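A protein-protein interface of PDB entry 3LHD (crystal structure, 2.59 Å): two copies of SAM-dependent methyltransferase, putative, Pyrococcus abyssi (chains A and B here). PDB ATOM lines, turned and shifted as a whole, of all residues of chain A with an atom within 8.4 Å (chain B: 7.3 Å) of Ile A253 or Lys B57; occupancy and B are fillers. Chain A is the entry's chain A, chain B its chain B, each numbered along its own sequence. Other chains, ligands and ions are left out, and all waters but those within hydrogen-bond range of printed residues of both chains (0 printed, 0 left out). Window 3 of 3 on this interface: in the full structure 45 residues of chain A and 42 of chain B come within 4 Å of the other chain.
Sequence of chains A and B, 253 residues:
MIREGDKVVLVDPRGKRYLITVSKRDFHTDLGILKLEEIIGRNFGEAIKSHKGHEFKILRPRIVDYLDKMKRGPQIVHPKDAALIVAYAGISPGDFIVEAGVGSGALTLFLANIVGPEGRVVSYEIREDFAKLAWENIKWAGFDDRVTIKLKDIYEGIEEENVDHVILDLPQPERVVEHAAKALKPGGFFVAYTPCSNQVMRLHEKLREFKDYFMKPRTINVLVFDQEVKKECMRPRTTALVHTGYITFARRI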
ATOM      1  N   ALA A 181      27.564  -1.374   7.456  1.00  0.00           N
ATOM      2  CA  ALA A 181      26.888  -2.307   8.341  1.00  0.00           C
ATOM      3  C   ALA A 181      25.661  -2.922   7.684  1.00  0.00           C
ATOM      4  O   ALA A 181      25.283  -4.052   8.009  1.00  0.00           O
ATOM      5  CB  ALA A 181      26.493  -1.610   9.616  1.00  0.00           C
ATOM      6  N   LEU A 184      27.334  -5.067   4.165  1.00  0.00           N
ATOM      7  CA  LEU A 184      28.226  -6.221   4.325  1.00  0.00           C
ATOM      8  C   LEU A 184      27.544  -7.531   4.730  1.00  0.00           C
ATOM      9  O   LEU A 184      26.667  -7.526   5.589  1.00  0.00           O
ATOM     10  CB  LEU A 184      29.344  -5.891   5.326  1.00  0.00           C
ATOM     11  CG  LEU A 184      30.406  -4.887   4.867  1.00  0.00           C
ATOM     12  CD1 LEU A 184      31.059  -4.254   6.062  1.00  0.00           C
ATOM     13  CD2 LEU A 184      31.444  -5.554   3.983  1.00  0.00           C
ATOM     14  N   LYS A 185      27.958  -8.639   4.109  1.00  0.00           N
ATOM     15  CA  LYS A 185      27.596  -9.996   4.548  1.00  0.00           C
ATOM     16  C   LYS A 185      28.040 -10.228   5.990  1.00  0.00           C
ATOM     17  O   LYS A 185      29.036  -9.648   6.422  1.00  0.00           O
ATOM     18  CB  LYS A 185      28.361 -11.064   3.752  1.00  0.00           C
ATOM     19  CG  LYS A 185      28.060 -11.247   2.301  1.00  0.00           C
ATOM     20  CD  LYS A 185      29.015 -12.317   1.781  1.00  0.00           C
ATOM     21  CE  LYS A 185      29.176 -12.284   0.261  1.00  0.00           C
ATOM     22  NZ  LYS A 185      28.637 -13.498  -0.404  1.00  0.00           N
ATOM     23  N   PRO A 186      27.352 -11.132   6.718  1.00  0.00           N
ATOM     24  CA  PRO A 186      27.925 -11.630   7.972  1.00  0.00           C
ATOM     25  C   PRO A 186      29.364 -12.125   7.756  1.00  0.00           C
ATOM     26  O   PRO A 186      29.613 -12.928   6.849  1.00  0.00           O
ATOM     27  CB  PRO A 186      27.004 -12.801   8.336  1.00  0.00           C
ATOM     28  CG  PRO A 186      25.708 -12.477   7.692  1.00  0.00           C
ATOM     29  CD  PRO A 186      26.053 -11.763   6.417  1.00  0.00           C
ATOM     30  N   GLY A 187      30.297 -11.611   8.560  1.00  0.00           N
ATOM     31  CA  GLY A 187      31.715 -11.954   8.458  1.00  0.00           C
ATOM     32  C   GLY A 187      32.492 -11.106   7.467  1.00  0.00           C
ATOM     33  O   GLY A 187      33.677 -11.347   7.223  1.00  0.00           O
ATOM     34  N   GLY A 188      31.823 -10.114   6.886  1.00  0.00           N
ATOM     35  CA  GLY A 188      32.465  -9.187   5.945  1.00  0.00           C
ATOM     36  C   GLY A 188      33.364  -8.180   6.642  1.00  0.00           C
ATOM     37  O   GLY A 188      33.331  -8.037   7.869  1.00  0.00           O
ATOM     38  N   PHE A 189      34.170  -7.472   5.863  1.00  0.00           N
ATOM     39  CA  PHE A 189      35.132  -6.560   6.443  1.00  0.00           C
ATOM     40  C   PHE A 189      34.895  -5.123   6.016  1.00  0.00           C
ATOM     41  O   PHE A 189      34.721  -4.816   4.822  1.00  0.00           O
ATOM     42  CB  PHE A 189      36.567  -6.976   6.096  1.00  0.00           C
ATOM     43  CG  PHE A 189      37.184  -7.971   7.058  1.00  0.00           C
ATOM     44  CD1 PHE A 189      37.084  -9.339   6.827  1.00  0.00           C
ATOM     45  CD2 PHE A 189      37.898  -7.534   8.172  1.00  0.00           C
ATOM     46  CE1 PHE A 189      37.661 -10.265   7.706  1.00  0.00           C
ATOM     47  CE2 PHE A 189      38.484  -8.449   9.054  1.00  0.00           C
ATOM     48  CZ  PHE A 189      38.373  -9.819   8.814  1.00  0.00           C
ATOM     49  N   PHE A 210      29.049   1.454  17.022  1.00  0.00           N
ATOM     50  CA  PHE A 210      28.492   0.336  16.281  1.00  0.00           C
ATOM     51  C   PHE A 210      29.076  -1.022  16.700  1.00  0.00           C
ATOM     52  O   PHE A 210      29.230  -1.927  15.872  1.00  0.00           O
ATOM     53  CB  PHE A 210      28.644   0.586  14.779  1.00  0.00           C
ATOM     54  CG  PHE A 210      27.657   1.578  14.238  1.00  0.00           C
ATOM     55  CD1 PHE A 210      27.878   2.947  14.371  1.00  0.00           C
ATOM     56  CD2 PHE A 210      26.494   1.144  13.606  1.00  0.00           C
ATOM     57  CE1 PHE A 210      26.957   3.872  13.877  1.00  0.00           C
ATOM     58  CE2 PHE A 210      25.565   2.063  13.107  1.00  0.00           C
ATOM     59  CZ  PHE A 210      25.798   3.428  13.241  1.00  0.00           C
ATOM     60  N   LYS A 211      29.375  -1.158  17.992  1.00  0.00           N
ATOM     61  CA  LYS A 211      29.845  -2.421  18.574  1.00  0.00           C
ATOM     62  C   LYS A 211      28.894  -3.605  18.346  1.00  0.00           C
ATOM     63  O   LYS A 211      29.322  -4.754  18.383  1.00  0.00           O
ATOM     64  CB  LYS A 211      30.127  -2.247  20.070  1.00  0.00           C
ATOM     65  N   ASP A 212      27.611  -3.318  18.117  1.00  0.00           N
ATOM     66  CA  ASP A 212      26.598  -4.353  17.859  1.00  0.00           C
ATOM     67  C   ASP A 212      26.550  -4.811  16.392  1.00  0.00           C
ATOM     68  O   ASP A 212      25.832  -5.762  16.047  1.00  0.00           O
ATOM     69  CB  ASP A 212      25.209  -3.862  18.288  1.00  0.00           C
ATOM     70  CG  ASP A 212      25.068  -3.726  19.798  1.00  0.00           C
ATOM     71  OD1 ASP A 212      25.709  -4.507  20.546  1.00  0.00           O
ATOM     72  OD2 ASP A 212      24.299  -2.834  20.234  1.00  0.00           O
ATOM     73  N   TYR A 213      27.304  -4.125  15.537  1.00  0.00           N
ATOM     74  CA  TYR A 213      27.352  -4.434  14.112  1.00  0.00           C
ATOM     75  C   TYR A 213      28.757  -4.872  13.662  1.00  0.00           C
ATOM     76  O   TYR A 213      28.953  -5.270  12.515  1.00  0.00           O
ATOM     77  CB  TYR A 213      26.899  -3.219  13.295  1.00  0.00           C
ATOM     78  CG  TYR A 213      25.453  -2.806  13.505  1.00  0.00           C
ATOM     79  CD1 TYR A 213      24.495  -3.025  12.510  1.00  0.00           C
ATOM     80  CD2 TYR A 213      25.043  -2.179  14.687  1.00  0.00           C
ATOM     81  CE1 TYR A 213      23.166  -2.648  12.690  1.00  0.00           C
ATOM     82  CE2 TYR A 213      23.716  -1.804  14.879  1.00  0.00           C
ATOM     83  CZ  TYR A 213      22.785  -2.039  13.877  1.00  0.00           C
ATOM     84  OH  TYR A 213      21.473  -1.664  14.062  1.00  0.00           O
ATOM     85  N   PHE A 214      29.722  -4.793  14.579  1.00  0.00           N
ATOM     86  CA  PHE A 214      31.134  -4.991  14.263  1.00  0.00           C
ATOM     87  C   PHE A 214      31.927  -5.551  15.443  1.00  0.00           C
ATOM     88  O   PHE A 214      31.714  -5.163  16.599  1.00  0.00           O
ATOM     89  CB  PHE A 214      31.776  -3.668  13.854  1.00  0.00           C
ATOM     90  CG  PHE A 214      31.452  -3.227  12.461  1.00  0.00           C
ATOM     91  CD1 PHE A 214      30.617  -2.142  12.244  1.00  0.00           C
ATOM     92  CD2 PHE A 214      32.011  -3.873  11.360  1.00  0.00           C
ATOM     93  CE1 PHE A 214      30.328  -1.713  10.958  1.00  0.00           C
ATOM     94  CE2 PHE A 214      31.730  -3.455  10.072  1.00  0.00           C
ATOM     95  CZ  PHE A 214      30.886  -2.376   9.868  1.00  0.00           C
ATOM     96  N   MET A 215      32.853  -6.454  15.137  1.00  0.00           N
ATOM     97  CA  MET A 215      33.827  -6.937  16.103  1.00  0.00           C
ATOM     98  C   MET A 215      34.820  -5.819  16.409  1.00  0.00           C
ATOM     99  O   MET A 215      34.950  -4.878  15.626  1.00  0.00           O
ATOM    100  CB  MET A 215      34.578  -8.139  15.527  1.00  0.00           C
ATOM    101  CG  MET A 215      33.908  -9.482  15.764  1.00  0.00           C
ATOM    102  SD  MET A 215      34.544 -10.786  14.674  1.00  0.00           S
ATOM    103  CE  MET A 215      36.311 -10.718  15.012  1.00  0.00           C
ATOM    104  N   LYS A 216      35.524  -5.929  17.539  1.00  0.00           N
ATOM    105  CA  LYS A 216      36.521  -4.932  17.930  1.00  0.00           C
ATOM    106  C   LYS A 216      37.498  -4.678  16.781  1.00  0.00           C
ATOM    107  O   LYS A 216      38.083  -5.614  16.241  1.00  0.00           O
ATOM    108  CB  LYS A 216      37.268  -5.363  19.199  1.00  0.00           C
ATOM    109  N   ALA A 250      37.516  -3.961  10.498  1.00  0.00           N
ATOM    110  CA  ALA A 250      36.490  -4.458  11.429  1.00  0.00           C
ATOM    111  C   ALA A 250      35.576  -5.480  10.753  1.00  0.00           C
ATOM    112  O   ALA A 250      35.077  -5.236   9.655  1.00  0.00           O
ATOM    113  CB  ALA A 250      35.665  -3.297  12.008  1.00  0.00           C
ATOM    114  N   ARG A 251      35.379  -6.624  11.411  1.00  0.00           N
ATOM    115  CA  ARG A 251      34.442  -7.667  10.951  1.00  0.00           C
ATOM    116  C   ARG A 251      32.991  -7.346  11.291  1.00  0.00           C
ATOM    117  O   ARG A 251      32.661  -7.080  12.449  1.00  0.00           O
ATOM    118  CB  ARG A 251      34.775  -9.018  11.584  1.00  0.00           C
ATOM    119  CG  ARG A 251      35.671  -9.914  10.783  1.00  0.00           C
ATOM    120  CD  ARG A 251      34.931 -11.074  10.139  1.00  0.00           C
ATOM    121  NE  ARG A 251      35.757 -12.283  10.152  1.00  0.00           N
ATOM    122  CZ  ARG A 251      35.620 -13.328   9.338  1.00  0.00           C
ATOM    123  NH1 ARG A 251      34.690 -13.359   8.398  1.00  0.00           N
ATOM    124  NH2 ARG A 251      36.435 -14.356   9.459  1.00  0.00           N
ATOM    125  N   ARG A 252      32.134  -7.412  10.276  1.00  0.00           N
ATOM    126  CA  ARG A 252      30.703  -7.193  10.432  1.00  0.00           C
ATOM    127  C   ARG A 252      30.023  -8.301  11.251  1.00  0.00           C
ATOM    128  O   ARG A 252      29.962  -9.454  10.827  1.00  0.00           O
ATOM    129  CB  ARG A 252      30.045  -7.062   9.059  1.00  0.00           C
ATOM    130  CG  ARG A 252      28.731  -6.293   9.047  1.00  0.00           C
ATOM    131  CD  ARG A 252      27.542  -7.203   9.215  1.00  0.00           C
ATOM    132  NE  ARG A 252      26.334  -6.611   8.653  1.00  0.00           N
ATOM    133  CZ  ARG A 252      25.192  -7.269   8.455  1.00  0.00           C
ATOM    134  NH1 ARG A 252      25.090  -8.556   8.780  1.00  0.00           N
ATOM    135  NH2 ARG A 252      24.148  -6.635   7.929  1.00  0.00           N
ATOM    136  N   ILE A 253      29.524  -7.910  12.423  1.00  0.00           N
ATOM    137  CA  ILE A 253      28.742  -8.737  13.361  1.00  0.00           C
ATOM    138  C   ILE A 253      29.373 -10.089  13.714  1.00  0.00           C
ATOM    139  O   ILE A 253      29.574 -10.387  14.897  1.00  0.00           O
ATOM    140  CB  ILE A 253      27.218  -8.830  12.966  1.00  0.00           C
ATOM    141  CG1 ILE A 253      26.334  -8.781  14.225  1.00  0.00           C
ATOM    142  CG2 ILE A 253      26.915 -10.046  12.035  1.00  0.00           C
ATOM    143  CD1 ILE A 253      24.817  -8.820  13.958  1.00  0.00           C
ATOM    144  OXT ILE A 253      29.713 -10.907  12.853  1.00  0.00           O
ATOM    145  N   VAL B   8      32.378 -24.254   9.958  1.00  0.00           N
ATOM    146  CA  VAL B   8      31.739 -23.022  10.387  1.00  0.00           C
ATOM    147  C   VAL B   8      32.591 -22.297  11.434  1.00  0.00           C
ATOM    148  O   VAL B   8      33.337 -22.937  12.192  1.00  0.00           O
ATOM    149  CB  VAL B   8      30.326 -23.335  10.937  1.00  0.00           C
ATOM    150  CG1 VAL B   8      29.989 -22.491  12.132  1.00  0.00           C
ATOM    151  CG2 VAL B   8      29.287 -23.160   9.850  1.00  0.00           C
ATOM    152  N   VAL B   9      32.494 -20.968  11.463  1.00  0.00           N
ATOM    153  CA  VAL B   9      33.170 -20.177  12.488  1.00  0.00           C
ATOM    154  C   VAL B   9      32.206 -19.711  13.575  1.00  0.00           C
ATOM    155  O   VAL B   9      31.280 -18.951  13.321  1.00  0.00           O
ATOM    156  CB  VAL B   9      33.910 -18.967  11.897  1.00  0.00           C
ATOM    157  CG1 VAL B   9      34.574 -18.160  13.002  1.00  0.00           C
ATOM    158  CG2 VAL B   9      34.953 -19.423  10.892  1.00  0.00           C
ATOM    159  N   LEU B  10      32.427 -20.187  14.792  1.00  0.00           N
ATOM    160  CA  LEU B  10      31.665 -19.714  15.930  1.00  0.00           C
ATOM    161  C   LEU B  10      32.410 -18.561  16.585  1.00  0.00           C
ATOM    162  O   LEU B  10      33.578 -18.699  16.947  1.00  0.00           O
ATOM    163  CB  LEU B  10      31.395 -20.855  16.919  1.00  0.00           C
ATOM    164  CG  LEU B  10      30.634 -22.047  16.324  1.00  0.00           C
ATOM    165  CD1 LEU B  10      30.352 -23.110  17.366  1.00  0.00           C
ATOM    166  CD2 LEU B  10      29.344 -21.608  15.642  1.00  0.00           C
ATOM    167  N   VAL B  11      31.739 -17.415  16.689  1.00  0.00           N
ATOM    168  CA  VAL B  11      32.283 -16.225  17.356  1.00  0.00           C
ATOM    169  C   VAL B  11      31.554 -16.037  18.685  1.00  0.00           C
ATOM    170  O   VAL B  11      30.326 -15.930  18.697  1.00  0.00           O
ATOM    171  CB  VAL B  11      32.101 -14.957  16.487  1.00  0.00           C
ATOM    172  CG1 VAL B  11      32.641 -13.726  17.195  1.00  0.00           C
ATOM    173  CG2 VAL B  11      32.767 -15.129  15.126  1.00  0.00           C
ATOM    174  N   ASP B  12      32.296 -15.998  19.794  1.00  0.00           N
ATOM    175  CA  ASP B  12      31.681 -15.778  21.108  1.00  0.00           C
ATOM    176  C   ASP B  12      31.560 -14.290  21.452  1.00  0.00           C
ATOM    177  O   ASP B  12      32.116 -13.457  20.737  1.00  0.00           O
ATOM    178  CB  ASP B  12      32.382 -16.599  22.212  1.00  0.00           C
ATOM    179  CG  ASP B  12      33.732 -16.014  22.660  1.00  0.00           C
ATOM    180  OD1 ASP B  12      34.382 -16.666  23.517  1.00  0.00           O
ATOM    181  OD2 ASP B  12      34.151 -14.931  22.180  1.00  0.00           O
ATOM    182  N   PRO B  13      30.817 -13.946  22.526  1.00  0.00           N
ATOM    183  CA  PRO B  13      30.620 -12.537  22.924  1.00  0.00           C
ATOM    184  C   PRO B  13      31.905 -11.708  23.040  1.00  0.00           C
ATOM    185  O   PRO B  13      31.895 -10.520  22.717  1.00  0.00           O
ATOM    186  CB  PRO B  13      29.947 -12.656  24.295  1.00  0.00           C
ATOM    187  CG  PRO B  13      29.169 -13.936  24.205  1.00  0.00           C
ATOM    188  CD  PRO B  13      29.994 -14.863  23.344  1.00  0.00           C
ATOM    189  N   LYS B  16      36.043 -13.996  20.370  1.00  0.00           N
ATOM    190  CA  LYS B  16      36.891 -15.161  20.110  1.00  0.00           C
ATOM    191  C   LYS B  16      36.268 -16.078  19.049  1.00  0.00           C
ATOM    192  O   LYS B  16      35.047 -16.261  19.012  1.00  0.00           O
ATOM    193  CB  LYS B  16      37.161 -15.946  21.402  1.00  0.00           C
ATOM    194  CG  LYS B  16      38.393 -16.836  21.333  1.00  0.00           C
ATOM    195  CD  LYS B  16      38.429 -17.874  22.441  1.00  0.00           C
ATOM    196  CE  LYS B  16      39.588 -18.856  22.224  1.00  0.00           C
ATOM    197  NZ  LYS B  16      39.683 -19.881  23.303  1.00  0.00           N
ATOM    198  N   TYR B  18      36.096 -19.883  16.870  1.00  0.00           N
ATOM    199  CA  TYR B  18      36.358 -21.316  16.869  1.00  0.00           C
ATOM    200  C   TYR B  18      35.978 -21.874  15.515  1.00  0.00           C
ATOM    201  O   TYR B  18      34.793 -21.905  15.162  1.00  0.00           O
ATOM    202  CB  TYR B  18      35.536 -22.046  17.923  1.00  0.00           C
ATOM    203  CG  TYR B  18      35.753 -21.603  19.343  1.00  0.00           C
ATOM    204  CD1 TYR B  18      36.516 -22.377  20.219  1.00  0.00           C
ATOM    205  CD2 TYR B  18      35.163 -20.427  19.832  1.00  0.00           C
ATOM    206  CE1 TYR B  18      36.706 -21.989  21.541  1.00  0.00           C
ATOM    207  CE2 TYR B  18      35.355 -20.027  21.149  1.00  0.00           C
ATOM    208  CZ  TYR B  18      36.126 -20.816  21.998  1.00  0.00           C
ATOM    209  OH  TYR B  18      36.320 -20.429  23.302  1.00  0.00           O
ATOM    210  N   ASN B  43      21.595 -20.770   9.478  1.00  0.00           N
ATOM    211  CA  ASN B  43      22.218 -20.103   8.345  1.00  0.00           C
ATOM    212  C   ASN B  43      23.319 -19.168   8.842  1.00  0.00           C
ATOM    213  O   ASN B  43      23.434 -18.924  10.043  1.00  0.00           O
ATOM    214  CB  ASN B  43      21.153 -19.357   7.531  1.00  0.00           C
ATOM    215  CG  ASN B  43      21.683 -18.809   6.216  1.00  0.00           C
ATOM    216  OD1 ASN B  43      22.633 -19.345   5.636  1.00  0.00           O
ATOM    217  ND2 ASN B  43      21.064 -17.725   5.735  1.00  0.00           N
ATOM    218  N   PHE B  44      24.154 -18.678   7.932  1.00  0.00           N
ATOM    219  CA  PHE B  44      25.218 -17.773   8.317  1.00  0.00           C
ATOM    220  C   PHE B  44      24.617 -16.445   8.702  1.00  0.00           C
ATOM    221  O   PHE B  44      23.805 -15.877   7.964  1.00  0.00           O
ATOM    222  CB  PHE B  44      26.249 -17.626   7.196  1.00  0.00           C
ATOM    223  CG  PHE B  44      26.996 -18.888   6.912  1.00  0.00           C
ATOM    224  CD1 PHE B  44      27.808 -19.459   7.884  1.00  0.00           C
ATOM    225  CD2 PHE B  44      26.873 -19.525   5.689  1.00  0.00           C
ATOM    226  CE1 PHE B  44      28.496 -20.635   7.643  1.00  0.00           C
ATOM    227  CE2 PHE B  44      27.566 -20.713   5.437  1.00  0.00           C
ATOM    228  CZ  PHE B  44      28.378 -21.264   6.419  1.00  0.00           C
ATOM    229  N   GLY B  45      24.998 -15.970   9.882  1.00  0.00           N
ATOM    230  CA  GLY B  45      24.464 -14.730  10.417  1.00  0.00           C
ATOM    231  C   GLY B  45      23.597 -15.004  11.618  1.00  0.00           C
ATOM    232  O   GLY B  45      23.199 -14.078  12.326  1.00  0.00           O
ATOM    233  N   GLU B  46      23.308 -16.282  11.844  1.00  0.00           N
ATOM    234  CA  GLU B  46      22.493 -16.714  12.975  1.00  0.00           C
ATOM    235  C   GLU B  46      23.357 -17.123  14.160  1.00  0.00           C
ATOM    236  O   GLU B  46      24.579 -17.077  14.094  1.00  0.00           O
ATOM    237  CB  GLU B  46      21.590 -17.883  12.579  1.00  0.00           C
ATOM    238  CG  GLU B  46      20.503 -17.558  11.586  1.00  0.00           C
ATOM    239  CD  GLU B  46      19.710 -18.792  11.208  1.00  0.00           C
ATOM    240  OE1 GLU B  46      19.392 -19.605  12.103  1.00  0.00           O
ATOM    241  OE2 GLU B  46      19.408 -18.963  10.014  1.00  0.00           O
ATOM    242  N   ALA B  47      22.710 -17.546  15.240  1.00  0.00           N
ATOM    243  CA  ALA B  47      23.416 -17.850  16.473  1.00  0.00           C
ATOM    244  C   ALA B  47      22.899 -19.095  17.166  1.00  0.00           C
ATOM    245  O   ALA B  47      21.781 -19.551  16.914  1.00  0.00           O
ATOM    246  CB  ALA B  47      23.372 -16.656  17.422  1.00  0.00           C
ATOM    247  N   ILE B  48      23.736 -19.639  18.043  1.00  0.00           N
ATOM    248  CA  ILE B  48      23.375 -20.776  18.867  1.00  0.00           C
ATOM    249  C   ILE B  48      23.839 -20.473  20.282  1.00  0.00           C
ATOM    250  O   ILE B  48      24.756 -19.676  20.472  1.00  0.00           O
ATOM    251  CB  ILE B  48      23.981 -22.100  18.305  1.00  0.00           C
ATOM    252  CG1 ILE B  48      23.202 -23.312  18.819  1.00  0.00           C
ATOM    253  CG2 ILE B  48      25.502 -22.218  18.570  1.00  0.00           C
ATOM    254  CD1 ILE B  48      23.592 -24.602  18.135  1.00  0.00           C
ATOM    255  N   GLU B  55      25.599 -16.690  23.743  1.00  0.00           N
ATOM    256  CA  GLU B  55      25.314 -16.802  22.309  1.00  0.00           C
ATOM    257  C   GLU B  55      26.562 -16.815  21.426  1.00  0.00           C
ATOM    258  O   GLU B  55      27.456 -15.982  21.574  1.00  0.00           O
ATOM    259  CB  GLU B  55      24.360 -15.690  21.860  1.00  0.00           C
ATOM    260  N   PHE B  56      26.603 -17.761  20.493  1.00  0.00           N
ATOM    261  CA  PHE B  56      27.709 -17.888  19.556  1.00  0.00           C
ATOM    262  C   PHE B  56      27.185 -17.644  18.155  1.00  0.00           C
ATOM    263  O   PHE B  56      26.275 -18.331  17.709  1.00  0.00           O
ATOM    264  CB  PHE B  56      28.323 -19.289  19.650  1.00  0.00           C
ATOM    265  CG  PHE B  56      29.156 -19.504  20.877  1.00  0.00           C
ATOM    266  CD1 PHE B  56      30.534 -19.664  20.772  1.00  0.00           C
ATOM    267  CD2 PHE B  56      28.572 -19.539  22.137  1.00  0.00           C
ATOM    268  CE1 PHE B  56      31.318 -19.859  21.900  1.00  0.00           C
ATOM    269  CE2 PHE B  56      29.342 -19.729  23.274  1.00  0.00           C
ATOM    270  CZ  PHE B  56      30.719 -19.891  23.157  1.00  0.00           C
ATOM    271  N   LYS B  57      27.752 -16.661  17.466  1.00  0.00           N
ATOM    272  CA  LYS B  57      27.311 -16.331  16.117  1.00  0.00           C
ATOM    273  C   LYS B  57      28.007 -17.217  15.098  1.00  0.00           C
ATOM    274  O   LYS B  57      29.133 -17.668  15.322  1.00  0.00           O
ATOM    275  CB  LYS B  57      27.530 -14.846  15.802  1.00  0.00           C
ATOM    276  CG  LYS B  57      26.726 -13.914  16.703  1.00  0.00           C
ATOM    277  CD  LYS B  57      26.508 -12.545  16.081  1.00  0.00           C
ATOM    278  CE  LYS B  57      25.157 -12.443  15.351  1.00  0.00           C
ATOM    279  NZ  LYS B  57      25.170 -13.134  14.033  1.00  0.00           N
ATOM    280  N   ILE B  58      27.321 -17.456  13.980  1.00  0.00           N
ATOM    281  CA  ILE B  58      27.775 -18.390  12.960  1.00  0.00           C
ATOM    282  C   ILE B  58      28.192 -17.650  11.703  1.00  0.00           C
ATOM    283  O   ILE B  58      27.353 -17.040  11.036  1.00  0.00           O
ATOM    284  CB  ILE B  58      26.672 -19.412  12.590  1.00  0.00           C
ATOM    285  CG1 ILE B  58      26.137 -20.131  13.830  1.00  0.00           C
ATOM    286  CG2 ILE B  58      27.197 -20.417  11.576  1.00  0.00           C
ATOM    287  CD1 ILE B  58      24.787 -20.822  13.609  1.00  0.00           C
ATOM    288  N   LEU B  59      29.481 -17.724  11.377  1.00  0.00           N
ATOM    289  CA  LEU B  59      30.026 -17.094  10.180  1.00  0.00           C
ATOM    290  C   LEU B  59      30.624 -18.104   9.204  1.00  0.00           C
ATOM    291  O   LEU B  59      31.080 -19.171   9.607  1.00  0.00           O
ATOM    292  CB  LEU B  59      31.113 -16.086  10.558  1.00  0.00           C
ATOM    293  CG  LEU B  59      30.851 -14.894  11.482  1.00  0.00           C
ATOM    294  CD1 LEU B  59      32.154 -14.127  11.605  1.00  0.00           C
ATOM    295  CD2 LEU B  59      29.744 -13.978  10.962  1.00  0.00           C
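The backbone carbonyl oxygen (O) of Val B11 sits at hydrogen-bond distance from the backbone NH (N) of Lys B57. The backbone NH (N) of Gly B45 sits at hydrogen-bond distance from the backbone carbonyl oxygen (O) of Ile B58 (2.8 Å). The backbone carbonyl oxygen (O) of Arg A252 sits at hydrogen-bond distance from the backbone NH (N) of Gly A187, at 3.1 Å. The backbone carbonyl oxygen (O) of Tyr A213 is in hydrogen-bond range of the backbone NH (N) of Ile A253, at 2.7 Å. O of Gly A187 is in hydrogen-bond range of NH1 of Arg A251. The backbone carbonyl oxygen (O) of Gly B45 sits at hydrogen-bond distance from the side-chain amino group (NZ) of Lys B57 (2.8 Å).
Among the printed residues, pairs that only touch across the chains: Gly A187 with Leu B59 (3.4 Å), Ile A253 with Leu B59 (3.6 Å), Pro A186 with Leu B59 (3.7 Å), Pro A186 with Gly B45 (3.7 Å), Ile A253 with Lys B57 (3.9 Å) and Pro A186 with Phe B44 (3.9 Å).
Printed residues of chain B within 4 Å of Pro A186: Phe B44 (3.9 Å), Gly B45 (3.7 Å) and Leu B59 (3.7 Å). Of the printed residues of chain B, Gly A187 touches Leu B59 (3.4 Å). Ile A253 touches just these residues of chain B: Lys B57 and Leu B59. Printed residues of chain A within 4 Å of Leu B59: Pro A186, Gly A187 and Ile A253. The nearest residue of chain A that does not touch Lys B57 is Pro A186 (6.0 Å).
Printed residues of chain B that touch a printed residue of chain A: Phe B44, Gly B45, Lys B57 and Leu B59. Hydrophobic or aromatic side chains of chain B within 4 Å of the printed part of chain A: Leu B59.
No position is printed for both chains.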
